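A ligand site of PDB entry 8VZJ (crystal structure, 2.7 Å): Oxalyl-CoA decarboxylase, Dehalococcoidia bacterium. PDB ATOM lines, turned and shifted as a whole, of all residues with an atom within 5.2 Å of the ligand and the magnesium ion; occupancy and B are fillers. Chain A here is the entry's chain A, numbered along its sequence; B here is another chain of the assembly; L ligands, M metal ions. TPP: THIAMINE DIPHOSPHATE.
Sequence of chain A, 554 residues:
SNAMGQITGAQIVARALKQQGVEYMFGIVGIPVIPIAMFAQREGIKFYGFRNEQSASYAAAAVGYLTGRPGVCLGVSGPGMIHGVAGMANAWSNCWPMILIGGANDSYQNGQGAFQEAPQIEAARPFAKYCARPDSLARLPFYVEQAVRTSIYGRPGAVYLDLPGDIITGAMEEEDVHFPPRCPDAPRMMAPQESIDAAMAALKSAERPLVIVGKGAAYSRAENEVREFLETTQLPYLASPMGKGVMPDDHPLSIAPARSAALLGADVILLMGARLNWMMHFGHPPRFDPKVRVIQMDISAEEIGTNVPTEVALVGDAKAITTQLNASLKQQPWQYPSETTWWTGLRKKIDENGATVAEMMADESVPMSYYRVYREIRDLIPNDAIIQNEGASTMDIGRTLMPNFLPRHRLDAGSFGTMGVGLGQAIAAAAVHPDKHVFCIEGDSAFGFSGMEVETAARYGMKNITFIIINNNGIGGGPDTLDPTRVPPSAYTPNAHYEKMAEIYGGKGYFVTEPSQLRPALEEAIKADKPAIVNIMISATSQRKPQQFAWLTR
The magnesium ion is bound by O2A of the ligand (2.0 Å), OD1 of Asn 472 (2.0 Å), O of Gly 474 (2.3 Å), O2B of the ligand (2.3 Å) and OD1 of Asp 444 (2.5 Å).
Gly 391 touches the ligand (CA to O1A, 3.5 Å).
CA of Gly 443 touches O1A of the ligand, at 3.5 Å.
CE2 of Phe 449 touches N1' of the ligand, 3.7 Å away.
Ile 475 touches the ligand (CG2 to C7, 3.6 Å).
CG2 of Ile 28 of chain B touches CM4 of the ligand (3.7 Å).
Val 29 of chain B touches the ligand (O to C7', 3.8 Å).
Val 76 of chain B touches the ligand.
Pro 79 of chain B touches the ligand (CB to CM2, 3.6 Å).
Gly 80 of chain B touches the ligand.
CE1 of His 83 of chain B touches CM2 of the ligand (3.6 Å).
Hydrophobic or aromatic side chains that line the ligand: Tyr 370, Ala 392, Met 419, Ala 446, Phe 449, Ile 475, Ile 28 of chain B, Val 76 of chain B, Pro 79 of chain B and His 83 of chain B.
Within 4 Å of the ligand: Tyr 370, Gly 391, Ala 392, Ser 393, Thr 394, Gly 417, Met 419, Gly 443, Asp 444, Ser 445, Ala 446, Phe 449, Asn 472, Gly 474, Ile 475, Gly 476, Ile 28 of chain B, Val 29 of chain B, Glu 53 of chain B, Val 76 of chain B, Pro 79 of chain B, Gly 80 of chain B, His 83 of chain B and Gln 116 of chain B.
The nearest printed residue that does not touch the ligand is Gly 30 of chain B (4.1 Å).
An oxygen (O2A) of the ligand sits close to the backbone NH (N) of Asp 444 (3.3 Å).
O3B of the ligand lies within hydrogen-bond range of N of Thr 394 (2.5 Å).
O3B of the ligand lies within hydrogen-bond range of OG1 of Thr 394.
A nitrogen (N1') of the ligand lies within hydrogen-bond range of the side-chain carboxylate of Glu 53 of chain B (2.8 Å).
An oxygen (O3B) of the ligand lies within hydrogen-bond range of the backbone NH (N) of Ser 393 (2.8 Å).
The backbone carbonyl oxygen (O) of Gly 417 is in hydrogen-bond range of a nitrogen (N4') of the ligand, 2.9 Å away.
The side-chain hydroxyl (OH) of Tyr 370 sits at hydrogen-bond distance from an oxygen (O3B) of the ligand.
N of Ser 445 sits close to O2A of the ligand.
An oxygen (O1B) of the ligand sits at hydrogen-bond distance from the backbone NH (N) of Gly 476 (3.0 Å).
The backbone NH of Ala 446 is in hydrogen-bond range of an oxygen (O1A) of the ligand, 3.2 Å away.
A nitrogen (N4') of the ligand sits close to the side-chain amide nitrogen of Gln 116 of chain B.
The backbone NH (N) of Met 419 sits at hydrogen-bond distance from a nitrogen (N3') of the ligand.
O3A of the ligand sits at hydrogen-bond distance from N of Ala 392 (3.3 Å).
The side-chain amide nitrogen of Asn 472 is in hydrogen-bond range of the side-chain hydroxyl of Tyr 370 (3.3 Å).
The side-chain amide nitrogen of Asn 472 lies close to the backbone NH of Gly 477, 3.0 Å away.
The backbone NH (N) of Asp 444 lies within hydrogen-bond range of the backbone carbonyl oxygen (O) of Ile 470 (3.4 Å).
N of Asn 473 lies within hydrogen-bond range of OD2 of Asp 444 (3.2 Å).
OE1 of Glu 53 of chain B is in hydrogen-bond range of ND1 of His 83 of chain B (3.5 Å).
The backbone carbonyl oxygen (O) of Gly 417 lies within hydrogen-bond range of the side-chain amide nitrogen (NE2) of Gln 116 of chain B (3.2 Å).
The backbone NH of Gly 443 lies within hydrogen-bond range of the backbone carbonyl oxygen of Glu 390, 3.1 Å away.
Merely in contact with the magnesium ion: Gly 476 (3.8 Å).
Of the 33 residues printed, 4 come within 4 Å of the magnesium ion.
The nearest printed residue that does not touch the magnesium ion is Ile 475 (4.3 Å).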
ATOM      1  N   TYR A 370      43.604  30.984 -22.473  1.00  0.00           N
ATOM      2  CA  TYR A 370      42.675  30.057 -23.110  1.00  0.00           C
ATOM      3  C   TYR A 370      43.135  29.704 -24.520  1.00  0.00           C
ATOM      4  O   TYR A 370      42.966  28.562 -24.964  1.00  0.00           O
ATOM      5  CB  TYR A 370      41.273  30.655 -23.151  1.00  0.00           C
ATOM      6  CG  TYR A 370      40.543  30.704 -21.830  1.00  0.00           C
ATOM      7  CD1 TYR A 370      39.764  29.641 -21.407  1.00  0.00           C
ATOM      8  CD2 TYR A 370      40.624  31.829 -21.018  1.00  0.00           C
ATOM      9  CE1 TYR A 370      39.091  29.682 -20.202  1.00  0.00           C
ATOM     10  CE2 TYR A 370      39.958  31.883 -19.810  1.00  0.00           C
ATOM     11  CZ  TYR A 370      39.191  30.809 -19.402  1.00  0.00           C
ATOM     12  OH  TYR A 370      38.518  30.850 -18.197  1.00  0.00           O
ATOM     13  N   GLU A 390      31.934  22.532 -21.399  1.00  0.00           N
ATOM     14  CA  GLU A 390      31.085  23.125 -20.381  1.00  0.00           C
ATOM     15  C   GLU A 390      31.884  24.119 -19.557  1.00  0.00           C
ATOM     16  O   GLU A 390      33.017  23.844 -19.166  1.00  0.00           O
ATOM     17  CB  GLU A 390      30.483  22.051 -19.469  1.00  0.00           C
ATOM     18  CG  GLU A 390      29.410  22.572 -18.523  1.00  0.00           C
ATOM     19  CD  GLU A 390      28.875  21.496 -17.582  1.00  0.00           C
ATOM     20  OE1 GLU A 390      29.685  20.666 -17.113  1.00  0.00           O
ATOM     21  OE2 GLU A 390      27.656  21.493 -17.315  1.00  0.00           O
ATOM     22  N   GLY A 391      31.279  25.268 -19.291  1.00  0.00           N
ATOM     23  CA  GLY A 391      31.909  26.311 -18.511  1.00  0.00           C
ATOM     24  C   GLY A 391      31.412  27.674 -18.947  1.00  0.00           C
ATOM     25  O   GLY A 391      30.377  27.779 -19.599  1.00  0.00           O
ATOM     26  N   ALA A 392      32.151  28.704 -18.555  1.00  0.00           N
ATOM     27  CA  ALA A 392      31.837  30.067 -18.976  1.00  0.00           C
ATOM     28  C   ALA A 392      32.717  30.460 -20.158  1.00  0.00           C
ATOM     29  O   ALA A 392      32.400  30.159 -21.309  1.00  0.00           O
ATOM     30  CB  ALA A 392      32.018  31.046 -17.819  1.00  0.00           C
ATOM     31  N   SER A 393      33.835  31.139 -19.876  1.00  0.00           N
ATOM     32  CA  SER A 393      34.784  31.465 -20.933  1.00  0.00           C
ATOM     33  C   SER A 393      35.342  30.199 -21.570  1.00  0.00           C
ATOM     34  O   SER A 393      35.565  30.161 -22.786  1.00  0.00           O
ATOM     35  CB  SER A 393      35.916  32.328 -20.383  1.00  0.00           C
ATOM     36  OG  SER A 393      35.454  33.618 -20.027  1.00  0.00           O
ATOM     37  N   THR A 394      35.559  29.160 -20.768  1.00  0.00           N
ATOM     38  CA  THR A 394      36.049  27.887 -21.306  1.00  0.00           C
ATOM     39  C   THR A 394      35.116  27.349 -22.380  1.00  0.00           C
ATOM     40  O   THR A 394      35.574  26.826 -23.401  1.00  0.00           O
ATOM     41  CB  THR A 394      36.199  26.871 -20.172  1.00  0.00           C
ATOM     42  OG1 THR A 394      37.098  27.375 -19.186  1.00  0.00           O
ATOM     43  CG2 THR A 394      36.729  25.544 -20.707  1.00  0.00           C
ATOM     44  N   MET A 395      33.805  27.500 -22.186  1.00  0.00           N
ATOM     45  CA  MET A 395      32.840  27.004 -23.165  1.00  0.00           C
ATOM     46  C   MET A 395      32.703  27.952 -24.346  1.00  0.00           C
ATOM     47  O   MET A 395      32.575  27.506 -25.495  1.00  0.00           O
ATOM     48  CB  MET A 395      31.487  26.780 -22.502  1.00  0.00           C
ATOM     49  CG  MET A 395      30.451  26.108 -23.387  1.00  0.00           C
ATOM     50  SD  MET A 395      28.879  25.899 -22.541  1.00  0.00           S
ATOM     51  CE  MET A 395      28.459  27.605 -22.179  1.00  0.00           C
ATOM     52  N   GLY A 417      21.701  26.954 -20.427  1.00  0.00           N
ATOM     53  CA  GLY A 417      22.945  27.409 -19.804  1.00  0.00           C
ATOM     54  C   GLY A 417      23.301  26.634 -18.560  1.00  0.00           C
ATOM     55  O   GLY A 417      23.761  27.229 -17.570  1.00  0.00           O
ATOM     56  N   THR A 418      23.105  25.322 -18.571  1.00  0.00           N
ATOM     57  CA  THR A 418      23.180  24.520 -17.364  1.00  0.00           C
ATOM     58  C   THR A 418      24.609  24.144 -17.036  1.00  0.00           C
ATOM     59  O   THR A 418      25.372  23.722 -17.916  1.00  0.00           O
ATOM     60  CB  THR A 418      22.339  23.248 -17.526  1.00  0.00           C
ATOM     61  OG1 THR A 418      21.024  23.594 -17.994  1.00  0.00           O
ATOM     62  CG2 THR A 418      22.226  22.519 -16.200  1.00  0.00           C
ATOM     63  N   MET A 419      24.979  24.290 -15.766  1.00  0.00           N
ATOM     64  CA  MET A 419      26.209  23.718 -15.234  1.00  0.00           C
ATOM     65  C   MET A 419      25.870  22.404 -14.540  1.00  0.00           C
ATOM     66  O   MET A 419      24.905  22.347 -13.771  1.00  0.00           O
ATOM     67  CB  MET A 419      26.904  24.682 -14.273  1.00  0.00           C
ATOM     68  CG  MET A 419      27.519  25.906 -14.939  1.00  0.00           C
ATOM     69  SD  MET A 419      28.760  25.496 -16.176  1.00  0.00           S
ATOM     70  CE  MET A 419      27.853  25.822 -17.692  1.00  0.00           C
ATOM     71  N   GLY A 443      35.533  23.655 -17.401  1.00  0.00           N
ATOM     72  CA  GLY A 443      36.097  24.595 -16.470  1.00  0.00           C
ATOM     73  C   GLY A 443      36.195  23.996 -15.083  1.00  0.00           C
ATOM     74  O   GLY A 443      35.485  23.048 -14.740  1.00  0.00           O
ATOM     75  N   ASP A 444      37.103  24.556 -14.269  1.00  0.00           N
ATOM     76  CA  ASP A 444      37.292  24.011 -12.924  1.00  0.00           C
ATOM     77  C   ASP A 444      36.018  24.125 -12.089  1.00  0.00           C
ATOM     78  O   ASP A 444      35.763  23.273 -11.237  1.00  0.00           O
ATOM     79  CB  ASP A 444      38.463  24.711 -12.227  1.00  0.00           C
ATOM     80  CG  ASP A 444      38.331  26.218 -12.232  1.00  0.00           C
ATOM     81  OD1 ASP A 444      37.942  26.771 -13.277  1.00  0.00           O
ATOM     82  OD2 ASP A 444      38.625  26.847 -11.202  1.00  0.00           O
ATOM     83  N   SER A 445      35.218  25.166 -12.318  1.00  0.00           N
ATOM     84  CA  SER A 445      33.941  25.287 -11.625  1.00  0.00           C
ATOM     85  C   SER A 445      32.939  24.269 -12.150  1.00  0.00           C
ATOM     86  O   SER A 445      32.270  23.582 -11.376  1.00  0.00           O
ATOM     87  CB  SER A 445      33.386  26.699 -11.760  1.00  0.00           C
ATOM     88  OG  SER A 445      32.109  26.816 -11.148  1.00  0.00           O
ATOM     89  N   ALA A 446      32.837  24.150 -13.484  1.00  0.00           N
ATOM     90  CA  ALA A 446      31.883  23.224 -14.077  1.00  0.00           C
ATOM     91  C   ALA A 446      32.195  21.778 -13.712  1.00  0.00           C
ATOM     92  O   ALA A 446      31.285  20.962 -13.552  1.00  0.00           O
ATOM     93  CB  ALA A 446      31.850  23.400 -15.592  1.00  0.00           C
ATOM     94  N   PHE A 449      30.577  20.216 -10.438  1.00  0.00           N
ATOM     95  CA  PHE A 449      29.152  19.904 -10.372  1.00  0.00           C
ATOM     96  C   PHE A 449      28.897  18.402 -10.445  1.00  0.00           C
ATOM     97  O   PHE A 449      27.965  17.905  -9.800  1.00  0.00           O
ATOM     98  CB  PHE A 449      28.397  20.613 -11.490  1.00  0.00           C
ATOM     99  CG  PHE A 449      28.172  22.071 -11.245  1.00  0.00           C
ATOM    100  CD1 PHE A 449      29.180  22.997 -11.492  1.00  0.00           C
ATOM    101  CD2 PHE A 449      26.953  22.528 -10.777  1.00  0.00           C
ATOM    102  CE1 PHE A 449      28.978  24.343 -11.264  1.00  0.00           C
ATOM    103  CE2 PHE A 449      26.739  23.881 -10.556  1.00  0.00           C
ATOM    104  CZ  PHE A 449      27.752  24.788 -10.799  1.00  0.00           C
ATOM    105  N   ILE A 470      40.283  23.036 -17.646  1.00  0.00           N
ATOM    106  CA  ILE A 470      40.922  24.337 -17.836  1.00  0.00           C
ATOM    107  C   ILE A 470      40.682  25.122 -16.548  1.00  0.00           C
ATOM    108  O   ILE A 470      39.583  25.627 -16.314  1.00  0.00           O
ATOM    109  CB  ILE A 470      40.386  25.054 -19.069  1.00  0.00           C
ATOM    110  CG1 ILE A 470      40.694  24.228 -20.327  1.00  0.00           C
ATOM    111  CG2 ILE A 470      40.996  26.434 -19.188  1.00  0.00           C
ATOM    112  CD1 ILE A 470      40.230  24.879 -21.607  1.00  0.00           C
ATOM    113  N   ASN A 472      41.209  28.031 -13.865  1.00  0.00           N
ATOM    114  CA  ASN A 472      41.574  29.410 -13.559  1.00  0.00           C
ATOM    115  C   ASN A 472      41.300  29.761 -12.097  1.00  0.00           C
ATOM    116  O   ASN A 472      41.203  30.941 -11.753  1.00  0.00           O
ATOM    117  CB  ASN A 472      40.842  30.376 -14.488  1.00  0.00           C
ATOM    118  CG  ASN A 472      39.338  30.263 -14.373  1.00  0.00           C
ATOM    119  OD1 ASN A 472      38.811  29.327 -13.771  1.00  0.00           O
ATOM    120  ND2 ASN A 472      38.627  31.229 -14.964  1.00  0.00           N
ATOM    121  N   ASN A 473      41.164  28.748 -11.237  1.00  0.00           N
ATOM    122  CA  ASN A 473      41.066  28.916  -9.791  1.00  0.00           C
ATOM    123  C   ASN A 473      39.814  29.689  -9.380  1.00  0.00           C
ATOM    124  O   ASN A 473      39.833  30.480  -8.439  1.00  0.00           O
ATOM    125  CB  ASN A 473      42.316  29.601  -9.222  1.00  0.00           C
ATOM    126  CG  ASN A 473      43.512  28.670  -9.159  1.00  0.00           C
ATOM    127  OD1 ASN A 473      43.363  27.451  -9.054  1.00  0.00           O
ATOM    128  ND2 ASN A 473      44.712  29.237  -9.207  1.00  0.00           N
ATOM    129  N   GLY A 474      38.705  29.441 -10.060  1.00  0.00           N
ATOM    130  CA  GLY A 474      37.449  30.027  -9.643  1.00  0.00           C
ATOM    131  C   GLY A 474      36.451  30.130 -10.773  1.00  0.00           C
ATOM    132  O   GLY A 474      36.690  29.677 -11.890  1.00  0.00           O
ATOM    133  N   ILE A 475      35.321  30.749 -10.445  1.00  0.00           N
ATOM    134  CA  ILE A 475      34.264  31.035 -11.409  1.00  0.00           C
ATOM    135  C   ILE A 475      34.659  32.314 -12.138  1.00  0.00           C
ATOM    136  O   ILE A 475      34.525  33.416 -11.604  1.00  0.00           O
ATOM    137  CB  ILE A 475      32.891  31.174 -10.727  1.00  0.00           C
ATOM    138  CG1 ILE A 475      32.519  29.878 -10.007  1.00  0.00           C
ATOM    139  CG2 ILE A 475      31.829  31.573 -11.745  1.00  0.00           C
ATOM    140  CD1 ILE A 475      31.155  29.921  -9.350  1.00  0.00           C
ATOM    141  N   GLY A 476      35.159  32.169 -13.359  1.00  0.00           N
ATOM    142  CA  GLY A 476      35.659  33.327 -14.080  1.00  0.00           C
ATOM    143  C   GLY A 476      36.960  33.873 -13.543  1.00  0.00           C
ATOM    144  O   GLY A 476      37.288  35.029 -13.819  1.00  0.00           O
ATOM    145  N   GLY A 477      37.698  33.077 -12.781  1.00  0.00           N
ATOM    146  CA  GLY A 477      38.956  33.524 -12.219  1.00  0.00           C
ATOM    147  C   GLY A 477      38.971  33.542 -10.700  1.00  0.00           C
ATOM    148  O   GLY A 477      37.915  33.534 -10.069  1.00  0.00           O
ATOM    149  N   ILE B  28      25.857  28.767  -5.178  1.00  0.00           N
ATOM    150  CA  ILE B  28      26.842  29.052  -6.212  1.00  0.00           C
ATOM    151  C   ILE B  28      26.455  30.365  -6.894  1.00  0.00           C
ATOM    152  O   ILE B  28      25.278  30.580  -7.216  1.00  0.00           O
ATOM    153  CB  ILE B  28      26.925  27.915  -7.241  1.00  0.00           C
ATOM    154  CG1 ILE B  28      27.264  26.606  -6.541  1.00  0.00           C
ATOM    155  CG2 ILE B  28      27.973  28.231  -8.298  1.00  0.00           C
ATOM    156  CD1 ILE B  28      27.266  25.411  -7.440  1.00  0.00           C
ATOM    157  N   VAL B  29      27.443  31.233  -7.093  1.00  0.00           N
ATOM    158  CA  VAL B  29      27.204  32.543  -7.675  1.00  0.00           C
ATOM    159  C   VAL B  29      27.024  32.418  -9.183  1.00  0.00           C
ATOM    160  O   VAL B  29      27.338  31.386  -9.777  1.00  0.00           O
ATOM    161  CB  VAL B  29      28.342  33.525  -7.348  1.00  0.00           C
ATOM    162  CG1 VAL B  29      28.498  33.655  -5.843  1.00  0.00           C
ATOM    163  CG2 VAL B  29      29.641  33.055  -7.989  1.00  0.00           C
ATOM    164  N   GLY B  30      26.527  33.478  -9.803  1.00  0.00           N
ATOM    165  CA  GLY B  30      26.259  33.482 -11.229  1.00  0.00           C
ATOM    166  C   GLY B  30      25.166  34.475 -11.547  1.00  0.00           C
ATOM    167  O   GLY B  30      24.597  35.116 -10.668  1.00  0.00           O
ATOM    168  N   ILE B  31      24.880  34.570 -12.848  1.00  0.00           N
ATOM    169  CA  ILE B  31      23.847  35.510 -13.303  1.00  0.00           C
ATOM    170  C   ILE B  31      22.499  35.083 -12.745  1.00  0.00           C
ATOM    171  O   ILE B  31      22.104  33.909 -12.903  1.00  0.00           O
ATOM    172  CB  ILE B  31      23.814  35.556 -14.848  1.00  0.00           C
ATOM    173  CG1 ILE B  31      25.186  35.937 -15.402  1.00  0.00           C
ATOM    174  CG2 ILE B  31      22.745  36.536 -15.326  1.00  0.00           C
ATOM    175  CD1 ILE B  31      25.642  37.321 -15.007  1.00  0.00           C
ATOM    176  N   GLU B  53      24.457  23.128  -6.269  1.00  0.00           N
ATOM    177  CA  GLU B  53      23.350  23.695  -5.495  1.00  0.00           C
ATOM    178  C   GLU B  53      22.578  22.630  -4.731  1.00  0.00           C
ATOM    179  O   GLU B  53      21.935  22.944  -3.729  1.00  0.00           O
ATOM    180  CB  GLU B  53      22.389  24.456  -6.411  1.00  0.00           C
ATOM    181  CG  GLU B  53      22.903  25.805  -6.888  1.00  0.00           C
ATOM    182  CD  GLU B  53      23.547  25.721  -8.247  1.00  0.00           C
ATOM    183  OE1 GLU B  53      23.831  24.590  -8.715  1.00  0.00           O
ATOM    184  OE2 GLU B  53      23.755  26.790  -8.869  1.00  0.00           O
ATOM    185  N   VAL B  76      21.261  30.493  -9.031  1.00  0.00           N
ATOM    186  CA  VAL B  76      21.047  31.319 -10.217  1.00  0.00           C
ATOM    187  C   VAL B  76      19.695  30.989 -10.827  1.00  0.00           C
ATOM    188  O   VAL B  76      18.978  30.106 -10.341  1.00  0.00           O
ATOM    189  CB  VAL B  76      22.167  31.115 -11.255  1.00  0.00           C
ATOM    190  CG1 VAL B  76      23.525  31.328 -10.612  1.00  0.00           C
ATOM    191  CG2 VAL B  76      22.080  29.731 -11.873  1.00  0.00           C
ATOM    192  N   PRO B  79      18.461  26.527 -14.081  1.00  0.00           N
ATOM    193  CA  PRO B  79      19.101  25.305 -13.556  1.00  0.00           C
ATOM    194  C   PRO B  79      19.575  25.421 -12.118  1.00  0.00           C
ATOM    195  O   PRO B  79      19.448  24.467 -11.349  1.00  0.00           O
ATOM    196  CB  PRO B  79      20.273  25.094 -14.516  1.00  0.00           C
ATOM    197  CG  PRO B  79      19.864  25.761 -15.775  1.00  0.00           C
ATOM    198  CD  PRO B  79      19.029  26.945 -15.380  1.00  0.00           C
ATOM    199  N   GLY B  80      20.134  26.576 -11.734  1.00  0.00           N
ATOM    200  CA  GLY B  80      20.634  26.715 -10.374  1.00  0.00           C
ATOM    201  C   GLY B  80      19.550  26.597  -9.324  1.00  0.00           C
ATOM    202  O   GLY B  80      19.720  25.906  -8.321  1.00  0.00           O
ATOM    203  N   HIS B  83      18.078  22.912  -9.068  1.00  0.00           N
ATOM    204  CA  HIS B  83      18.924  22.034  -8.261  1.00  0.00           C
ATOM    205  C   HIS B  83      18.656  22.212  -6.776  1.00  0.00           C
ATOM    206  O   HIS B  83      18.800  21.258  -5.998  1.00  0.00           O
ATOM    207  CB  HIS B  83      20.399  22.274  -8.562  1.00  0.00           C
ATOM    208  CG  HIS B  83      20.812  21.896  -9.940  1.00  0.00           C
ATOM    209  ND1 HIS B  83      22.099  22.087 -10.408  1.00  0.00           N
ATOM    210  CD2 HIS B  83      20.122  21.328 -10.962  1.00  0.00           C
ATOM    211  CE1 HIS B  83      22.178  21.659 -11.656  1.00  0.00           C
ATOM    212  NE2 HIS B  83      20.997  21.193 -12.009  1.00  0.00           N
ATOM    213  N   PHE B 115      17.343  34.199 -20.860  1.00  0.00           N
ATOM    214  CA  PHE B 115      18.359  33.282 -20.369  1.00  0.00           C
ATOM    215  C   PHE B 115      17.875  32.621 -19.080  1.00  0.00           C
ATOM    216  O   PHE B 115      17.590  33.302 -18.093  1.00  0.00           O
ATOM    217  CB  PHE B 115      19.668  34.037 -20.128  1.00  0.00           C
ATOM    218  CG  PHE B 115      20.810  33.147 -19.704  1.00  0.00           C
ATOM    219  CD1 PHE B 115      21.314  32.184 -20.561  1.00  0.00           C
ATOM    220  CD2 PHE B 115      21.378  33.294 -18.445  1.00  0.00           C
ATOM    221  CE1 PHE B 115      22.362  31.373 -20.162  1.00  0.00           C
ATOM    222  CE2 PHE B 115      22.429  32.491 -18.055  1.00  0.00           C
ATOM    223  CZ  PHE B 115      22.919  31.526 -18.908  1.00  0.00           C
ATOM    224  N   GLN B 116      17.789  31.289 -19.107  1.00  0.00           N
ATOM    225  CA  GLN B 116      17.399  30.482 -17.942  1.00  0.00           C
ATOM    226  C   GLN B 116      15.992  30.850 -17.453  1.00  0.00           C
ATOM    227  O   GLN B 116      15.709  30.778 -16.258  1.00  0.00           O
ATOM    228  CB  GLN B 116      18.425  30.602 -16.817  1.00  0.00           C
ATOM    229  CG  GLN B 116      19.818  30.159 -17.241  1.00  0.00           C
ATOM    230  CD  GLN B 116      20.857  30.287 -16.144  1.00  0.00           C
ATOM    231  OE1 GLN B 116      20.757  31.146 -15.264  1.00  0.00           O
ATOM    232  NE2 GLN B 116      21.875  29.434 -16.190  1.00  0.00           N
HETATM  233  N1' TPP L   1      24.664  26.759 -11.504  1.00  0.00           N
HETATM  234  C2' TPP L   1      24.045  26.278 -12.593  1.00  0.00           C
HETATM  235  CM2 TPP L   1      23.241  25.031 -12.420  1.00  0.00           C
HETATM  236  N3' TPP L   1      24.086  26.812 -13.813  1.00  0.00           N
HETATM  237  C4' TPP L   1      24.807  27.938 -13.983  1.00  0.00           C
HETATM  238  N4' TPP L   1      24.847  28.460 -15.214  1.00  0.00           N
HETATM  239  C5' TPP L   1      25.490  28.539 -12.884  1.00  0.00           C
HETATM  240  C6' TPP L   1      25.367  27.880 -11.684  1.00  0.00           C
HETATM  241  C7' TPP L   1      26.318  29.788 -13.019  1.00  0.00           C
HETATM  242  N3  TPP L   1      27.522  29.595 -13.856  1.00  0.00           N
HETATM  243  C2  TPP L   1      27.592  29.918 -15.132  1.00  0.00           C
HETATM  244  S1  TPP L   1      29.080  29.556 -15.805  1.00  0.00           S
HETATM  245  C5  TPP L   1      29.648  28.925 -14.302  1.00  0.00           C
HETATM  246  C4  TPP L   1      28.687  29.015 -13.351  1.00  0.00           C
HETATM  247  CM4 TPP L   1      28.772  28.584 -11.933  1.00  0.00           C
HETATM  248  C6  TPP L   1      31.036  28.363 -14.153  1.00  0.00           C
HETATM  249  C7  TPP L   1      32.109  29.331 -14.597  1.00  0.00           C
HETATM  250  O7  TPP L   1      33.399  28.802 -14.194  1.00  0.00           O
HETATM  251  PA  TPP L   1      34.236  27.768 -15.048  1.00  0.00           P
HETATM  252  O1A TPP L   1      33.430  26.584 -15.403  1.00  0.00           O
HETATM  253  O2A TPP L   1      35.519  27.457 -14.276  1.00  0.00           O
HETATM  254  O3A TPP L   1      34.647  28.611 -16.331  1.00  0.00           O
HETATM  255  PB  TPP L   1      35.691  29.721 -16.762  1.00  0.00           P
HETATM  256  O1B TPP L   1      35.347  31.045 -16.175  1.00  0.00           O
HETATM  257  O2B TPP L   1      37.041  29.176 -16.288  1.00  0.00           O
HETATM  258  O3B TPP L   1      35.657  29.706 -18.293  1.00  0.00           O
HETATM  259 MG    MG M   1      36.889  28.864 -14.004  1.00  0.00          MG
